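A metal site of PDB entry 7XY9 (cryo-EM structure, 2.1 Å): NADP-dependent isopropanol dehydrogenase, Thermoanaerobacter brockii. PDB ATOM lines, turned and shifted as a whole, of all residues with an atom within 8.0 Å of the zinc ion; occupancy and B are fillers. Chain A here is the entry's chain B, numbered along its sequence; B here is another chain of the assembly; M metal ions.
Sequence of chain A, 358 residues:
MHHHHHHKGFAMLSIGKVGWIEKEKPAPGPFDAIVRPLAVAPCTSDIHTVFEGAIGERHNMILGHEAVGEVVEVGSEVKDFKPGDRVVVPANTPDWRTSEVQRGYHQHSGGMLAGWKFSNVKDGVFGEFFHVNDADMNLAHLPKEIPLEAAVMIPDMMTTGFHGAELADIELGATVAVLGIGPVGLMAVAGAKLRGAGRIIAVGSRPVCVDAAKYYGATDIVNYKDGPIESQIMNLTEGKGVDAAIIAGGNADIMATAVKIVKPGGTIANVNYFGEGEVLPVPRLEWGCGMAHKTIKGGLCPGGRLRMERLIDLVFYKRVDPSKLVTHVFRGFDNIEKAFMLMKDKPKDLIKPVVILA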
ATOM      1  N   ALA A  41      15.734  25.019 -10.239  1.00  0.00           N
ATOM      2  CA  ALA A  41      14.282  25.076 -10.244  1.00  0.00           C
ATOM      3  C   ALA A  41      13.728  24.411  -8.983  1.00  0.00           C
ATOM      4  O   ALA A  41      14.055  23.240  -8.718  1.00  0.00           O
ATOM      5  CB  ALA A  41      13.703  24.397 -11.492  1.00  0.00           C
ATOM      6  N   PRO A  42      12.916  25.119  -8.199  1.00  0.00           N
ATOM      7  CA  PRO A  42      12.246  24.471  -7.065  1.00  0.00           C
ATOM      8  C   PRO A  42      11.197  23.476  -7.534  1.00  0.00           C
ATOM      9  O   PRO A  42      10.663  23.559  -8.638  1.00  0.00           O
ATOM     10  CB  PRO A  42      11.604  25.647  -6.319  1.00  0.00           C
ATOM     11  CG  PRO A  42      11.439  26.698  -7.360  1.00  0.00           C
ATOM     12  CD  PRO A  42      12.603  26.556  -8.289  1.00  0.00           C
ATOM     13  N   CYS A  43      10.916  22.511  -6.664  1.00  0.00           N
ATOM     14  CA  CYS A  43       9.971  21.439  -6.967  1.00  0.00           C
ATOM     15  C   CYS A  43       8.943  21.328  -5.853  1.00  0.00           C
ATOM     16  O   CYS A  43       9.165  21.786  -4.724  1.00  0.00           O
ATOM     17  CB  CYS A  43      10.696  20.097  -7.162  1.00  0.00           C
ATOM     18  SG  CYS A  43       9.653  18.768  -7.793  1.00  0.00           S
ATOM     19  N   THR A  44       7.808  20.723  -6.184  1.00  0.00           N
ATOM     20  CA  THR A  44       6.777  20.466  -5.177  1.00  0.00           C
ATOM     21  C   THR A  44       7.276  19.478  -4.120  1.00  0.00           C
ATOM     22  O   THR A  44       6.762  19.474  -2.993  1.00  0.00           O
ATOM     23  CB  THR A  44       5.509  19.942  -5.836  1.00  0.00           C
ATOM     24  OG1 THR A  44       5.840  18.869  -6.727  1.00  0.00           O
ATOM     25  CG2 THR A  44       4.818  21.045  -6.623  1.00  0.00           C
ATOM     26  N   SER A  45       8.252  18.640  -4.473  1.00  0.00           N
ATOM     27  CA  SER A  45       8.811  17.697  -3.504  1.00  0.00           C
ATOM     28  C   SER A  45       9.489  18.433  -2.358  1.00  0.00           C
ATOM     29  O   SER A  45       9.381  18.026  -1.196  1.00  0.00           O
ATOM     30  CB  SER A  45       9.782  16.754  -4.196  1.00  0.00           C
ATOM     31  OG  SER A  45      11.038  17.368  -4.408  1.00  0.00           O
ATOM     32  N   ASP A  46      10.193  19.528  -2.659  1.00  0.00           N
ATOM     33  CA  ASP A  46      10.819  20.325  -1.609  1.00  0.00           C
ATOM     34  C   ASP A  46       9.773  20.886  -0.662  1.00  0.00           C
ATOM     35  O   ASP A  46       9.973  20.920   0.558  1.00  0.00           O
ATOM     36  CB  ASP A  46      11.652  21.448  -2.212  1.00  0.00           C
ATOM     37  CG  ASP A  46      12.815  20.942  -3.042  1.00  0.00           C
ATOM     38  OD1 ASP A  46      13.508  20.015  -2.583  1.00  0.00           O
ATOM     39  OD2 ASP A  46      13.025  21.475  -4.148  1.00  0.00           O
ATOM     40  N   GLY A  64      16.591  21.449  -2.909  1.00  0.00           N
ATOM     41  CA  GLY A  64      16.776  21.505  -4.343  1.00  0.00           C
ATOM     42  C   GLY A  64      17.391  20.262  -4.958  1.00  0.00           C
ATOM     43  O   GLY A  64      18.385  19.739  -4.446  1.00  0.00           O
ATOM     44  N   HIS A  65      16.809  19.769  -6.055  1.00  0.00           N
ATOM     45  CA  HIS A  65      17.374  18.616  -6.750  1.00  0.00           C
ATOM     46  C   HIS A  65      17.277  18.740  -8.270  1.00  0.00           C
ATOM     47  O   HIS A  65      17.366  17.719  -8.970  1.00  0.00           O
ATOM     48  CB  HIS A  65      16.705  17.321  -6.290  1.00  0.00           C
ATOM     49  CG  HIS A  65      15.283  17.170  -6.728  1.00  0.00           C
ATOM     50  ND1 HIS A  65      14.678  15.942  -6.860  1.00  0.00           N
ATOM     51  CD2 HIS A  65      14.351  18.102  -7.054  1.00  0.00           C
ATOM     52  CE1 HIS A  65      13.425  16.117  -7.261  1.00  0.00           C
ATOM     53  NE2 HIS A  65      13.211  17.419  -7.387  1.00  0.00           N
ATOM     54  N   GLU A  66      17.094  19.946  -8.802  1.00  0.00           N
ATOM     55  CA  GLU A  66      16.974  20.167 -10.244  1.00  0.00           C
ATOM     56  C   GLU A  66      17.912  21.313 -10.624  1.00  0.00           C
ATOM     57  O   GLU A  66      17.567  22.490 -10.444  1.00  0.00           O
ATOM     58  CB  GLU A  66      15.534  20.479 -10.648  1.00  0.00           C
ATOM     59  CG  GLU A  66      14.574  19.333 -10.437  1.00  0.00           C
ATOM     60  CD  GLU A  66      13.121  19.738 -10.651  1.00  0.00           C
ATOM     61  OE1 GLU A  66      12.852  20.514 -11.584  1.00  0.00           O
ATOM     62  OE2 GLU A  66      12.256  19.265  -9.885  1.00  0.00           O
ATOM     63  N   ALA A  91      18.416  14.340 -11.152  1.00  0.00           N
ATOM     64  CA  ALA A  91      17.887  14.361  -9.788  1.00  0.00           C
ATOM     65  C   ALA A  91      18.205  13.066  -9.051  1.00  0.00           C
ATOM     66  O   ALA A  91      18.482  13.081  -7.845  1.00  0.00           O
ATOM     67  CB  ALA A  91      16.381  14.613  -9.809  1.00  0.00           C
ATOM     68  N   TRP A 116      18.152   8.579  -4.893  1.00  0.00           N
ATOM     69  CA  TRP A 116      17.462   9.787  -4.460  1.00  0.00           C
ATOM     70  C   TRP A 116      18.212  10.340  -3.251  1.00  0.00           C
ATOM     71  O   TRP A 116      17.880  10.052  -2.100  1.00  0.00           O
ATOM     72  CB  TRP A 116      15.998   9.496  -4.151  1.00  0.00           C
ATOM     73  CG  TRP A 116      15.175   9.270  -5.371  1.00  0.00           C
ATOM     74  CD1 TRP A 116      14.571   8.108  -5.755  1.00  0.00           C
ATOM     75  CD2 TRP A 116      14.878  10.231  -6.400  1.00  0.00           C
ATOM     76  NE1 TRP A 116      13.906   8.278  -6.946  1.00  0.00           N
ATOM     77  CE2 TRP A 116      14.084   9.581  -7.365  1.00  0.00           C
ATOM     78  CE3 TRP A 116      15.199  11.576  -6.591  1.00  0.00           C
ATOM     79  CZ2 TRP A 116      13.604  10.221  -8.494  1.00  0.00           C
ATOM     80  CZ3 TRP A 116      14.718  12.216  -7.719  1.00  0.00           C
ATOM     81  CH2 TRP A 116      13.930  11.545  -8.660  1.00  0.00           C
ATOM     82  N   SER A 119      18.775  16.633  -1.337  1.00  0.00           N
ATOM     83  CA  SER A 119      17.767  17.166  -0.416  1.00  0.00           C
ATOM     84  C   SER A 119      16.989  16.070   0.306  1.00  0.00           C
ATOM     85  O   SER A 119      15.898  16.318   0.829  1.00  0.00           O
ATOM     86  CB  SER A 119      16.798  18.114  -1.145  1.00  0.00           C
ATOM     87  OG  SER A 119      15.874  17.396  -1.950  1.00  0.00           O
ATOM     88  N   PRO A 155      16.378  17.359 -15.690  1.00  0.00           N
ATOM     89  CA  PRO A 155      16.769  16.454 -14.587  1.00  0.00           C
ATOM     90  C   PRO A 155      15.634  15.708 -13.910  1.00  0.00           C
ATOM     91  O   PRO A 155      15.810  14.527 -13.570  1.00  0.00           O
ATOM     92  CB  PRO A 155      17.476  17.396 -13.605  1.00  0.00           C
ATOM     93  CG  PRO A 155      18.003  18.481 -14.453  1.00  0.00           C
ATOM     94  CD  PRO A 155      16.938  18.704 -15.477  1.00  0.00           C
ATOM     95  N   ASP A 156      14.483  16.344 -13.665  1.00  0.00           N
ATOM     96  CA  ASP A 156      13.393  15.644 -12.971  1.00  0.00           C
ATOM     97  C   ASP A 156      12.103  15.590 -13.781  1.00  0.00           C
ATOM     98  O   ASP A 156      11.568  14.500 -13.999  1.00  0.00           O
ATOM     99  CB  ASP A 156      13.145  16.288 -11.604  1.00  0.00           C
ATOM    100  CG  ASP A 156      12.377  15.374 -10.668  1.00  0.00           C
ATOM    101  OD1 ASP A 156      11.129  15.376 -10.712  1.00  0.00           O
ATOM    102  OD2 ASP A 156      13.024  14.647  -9.889  1.00  0.00           O
ATOM    103  N   MET A 157      11.583  16.738 -14.242  1.00  0.00           N
ATOM    104  CA  MET A 157      10.265  16.760 -14.868  1.00  0.00           C
ATOM    105  C   MET A 157      10.231  15.904 -16.136  1.00  0.00           C
ATOM    106  O   MET A 157       9.367  15.036 -16.296  1.00  0.00           O
ATOM    107  CB  MET A 157       9.858  18.193 -15.191  1.00  0.00           C
ATOM    108  CG  MET A 157      10.006  19.222 -14.067  1.00  0.00           C
ATOM    109  SD  MET A 157       8.796  19.061 -12.735  1.00  0.00           S
ATOM    110  CE  MET A 157       9.605  17.934 -11.612  1.00  0.00           C
ATOM    111  N   THR A 160      10.819  12.075 -15.464  1.00  0.00           N
ATOM    112  CA  THR A 160       9.684  11.420 -14.805  1.00  0.00           C
ATOM    113  C   THR A 160       8.511  11.261 -15.764  1.00  0.00           C
ATOM    114  O   THR A 160       7.909  10.184 -15.856  1.00  0.00           O
ATOM    115  CB  THR A 160       9.267  12.208 -13.558  1.00  0.00           C
ATOM    116  OG1 THR A 160      10.381  12.324 -12.678  1.00  0.00           O
ATOM    117  CG2 THR A 160       8.126  11.503 -12.835  1.00  0.00           C
ATOM    118  N   VAL A 184       4.889  17.503 -14.549  1.00  0.00           N
ATOM    119  CA  VAL A 184       5.122  16.095 -14.820  1.00  0.00           C
ATOM    120  C   VAL A 184       4.072  15.557 -15.779  1.00  0.00           C
ATOM    121  O   VAL A 184       4.383  14.774 -16.681  1.00  0.00           O
ATOM    122  CB  VAL A 184       5.173  15.295 -13.499  1.00  0.00           C
ATOM    123  CG1 VAL A 184       5.120  13.796 -13.767  1.00  0.00           C
ATOM    124  CG2 VAL A 184       6.413  15.647 -12.699  1.00  0.00           C
ATOM    125  N   TYR A 273       4.608  11.357  -7.505  1.00  0.00           N
ATOM    126  CA  TYR A 273       5.360  11.240  -6.270  1.00  0.00           C
ATOM    127  C   TYR A 273       4.559  11.802  -5.094  1.00  0.00           C
ATOM    128  O   TYR A 273       3.963  12.871  -5.186  1.00  0.00           O
ATOM    129  CB  TYR A 273       6.697  11.972  -6.387  1.00  0.00           C
ATOM    130  CG  TYR A 273       7.332  12.281  -5.048  1.00  0.00           C
ATOM    131  CD1 TYR A 273       7.912  11.283  -4.288  1.00  0.00           C
ATOM    132  CD2 TYR A 273       7.354  13.578  -4.554  1.00  0.00           C
ATOM    133  CE1 TYR A 273       8.501  11.568  -3.065  1.00  0.00           C
ATOM    134  CE2 TYR A 273       7.934  13.869  -3.339  1.00  0.00           C
ATOM    135  CZ  TYR A 273       8.503  12.862  -2.597  1.00  0.00           C
ATOM    136  OH  TYR A 273       9.083  13.153  -1.382  1.00  0.00           O
ATOM    137  N   LYS A 352       6.251  26.390 -13.636  1.00  0.00           N
ATOM    138  CA  LYS A 352       7.564  26.067 -13.115  1.00  0.00           C
ATOM    139  C   LYS A 352       8.460  27.310 -13.112  1.00  0.00           C
ATOM    140  O   LYS A 352       8.726  27.890 -14.180  1.00  0.00           O
ATOM    141  CB  LYS A 352       8.208  24.953 -13.946  1.00  0.00           C
ATOM    142  CG  LYS A 352       9.349  24.244 -13.251  1.00  0.00           C
ATOM    143  CD  LYS A 352       8.863  23.065 -12.431  1.00  0.00           C
ATOM    144  CE  LYS A 352      10.030  22.337 -11.787  1.00  0.00           C
ATOM    145  NZ  LYS A 352       9.623  21.536 -10.604  1.00  0.00           N
ATOM    146  N   TRP B 287      10.561   8.365  -1.814  1.00  0.00           N
ATOM    147  CA  TRP B 287      11.982   8.198  -2.100  1.00  0.00           C
ATOM    148  C   TRP B 287      12.600   7.092  -1.250  1.00  0.00           C
ATOM    149  O   TRP B 287      13.430   6.320  -1.731  1.00  0.00           O
ATOM    150  CB  TRP B 287      12.729   9.510  -1.869  1.00  0.00           C
ATOM    151  CG  TRP B 287      12.469  10.557  -2.914  1.00  0.00           C
ATOM    152  CD1 TRP B 287      12.011  10.347  -4.183  1.00  0.00           C
ATOM    153  CD2 TRP B 287      12.650  11.967  -2.766  1.00  0.00           C
ATOM    154  NE1 TRP B 287      11.902  11.552  -4.840  1.00  0.00           N
ATOM    155  CE2 TRP B 287      12.281  12.558  -3.990  1.00  0.00           C
ATOM    156  CE3 TRP B 287      13.086  12.790  -1.722  1.00  0.00           C
ATOM    157  CZ2 TRP B 287      12.343  13.937  -4.199  1.00  0.00           C
ATOM    158  CZ3 TRP B 287      13.140  14.157  -1.933  1.00  0.00           C
ATOM    159  CH2 TRP B 287      12.764  14.712  -3.162  1.00  0.00           C
HETATM  160 ZN    ZN M   1      11.577  17.444  -8.665  1.00  0.00          ZN
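The backbone carbonyl oxygen of Glu 66 lies within hydrogen-bond range of the backbone NH of Ala 41, at 3.1 Å. The side-chain carboxylate of Asp 46 lies within hydrogen-bond range of the backbone NH of Cys 43 (3.4 Å). The side-chain amino group (NZ) of Lys 352 is in salt-bridge range of the side-chain carboxylate (OE1) of Glu 66 (3.5 Å). OG1 of Thr 160 is in hydrogen-bond range of O of Asp 156 (2.8 Å). SG of Cys 43 sits close to N of Ser 45. SD of Met 157 sits at hydrogen-bond distance from NZ of Lys 352, at 3.4 Å.
Residues that only touch the zinc ion: Asp 156 (2.9 Å) and Met 157 (3.6 Å). Within 4 Å of the zinc ion: Cys 43, His 65, Glu 66, Asp 156 and Met 157.
NE2 of His 65 binds the zinc ion (2.1 Å). OE2 of Glu 66 is bound to the zinc ion (2.3 Å). The side-chain sulfur (SG) of Cys 43 is bound to the zinc ion.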
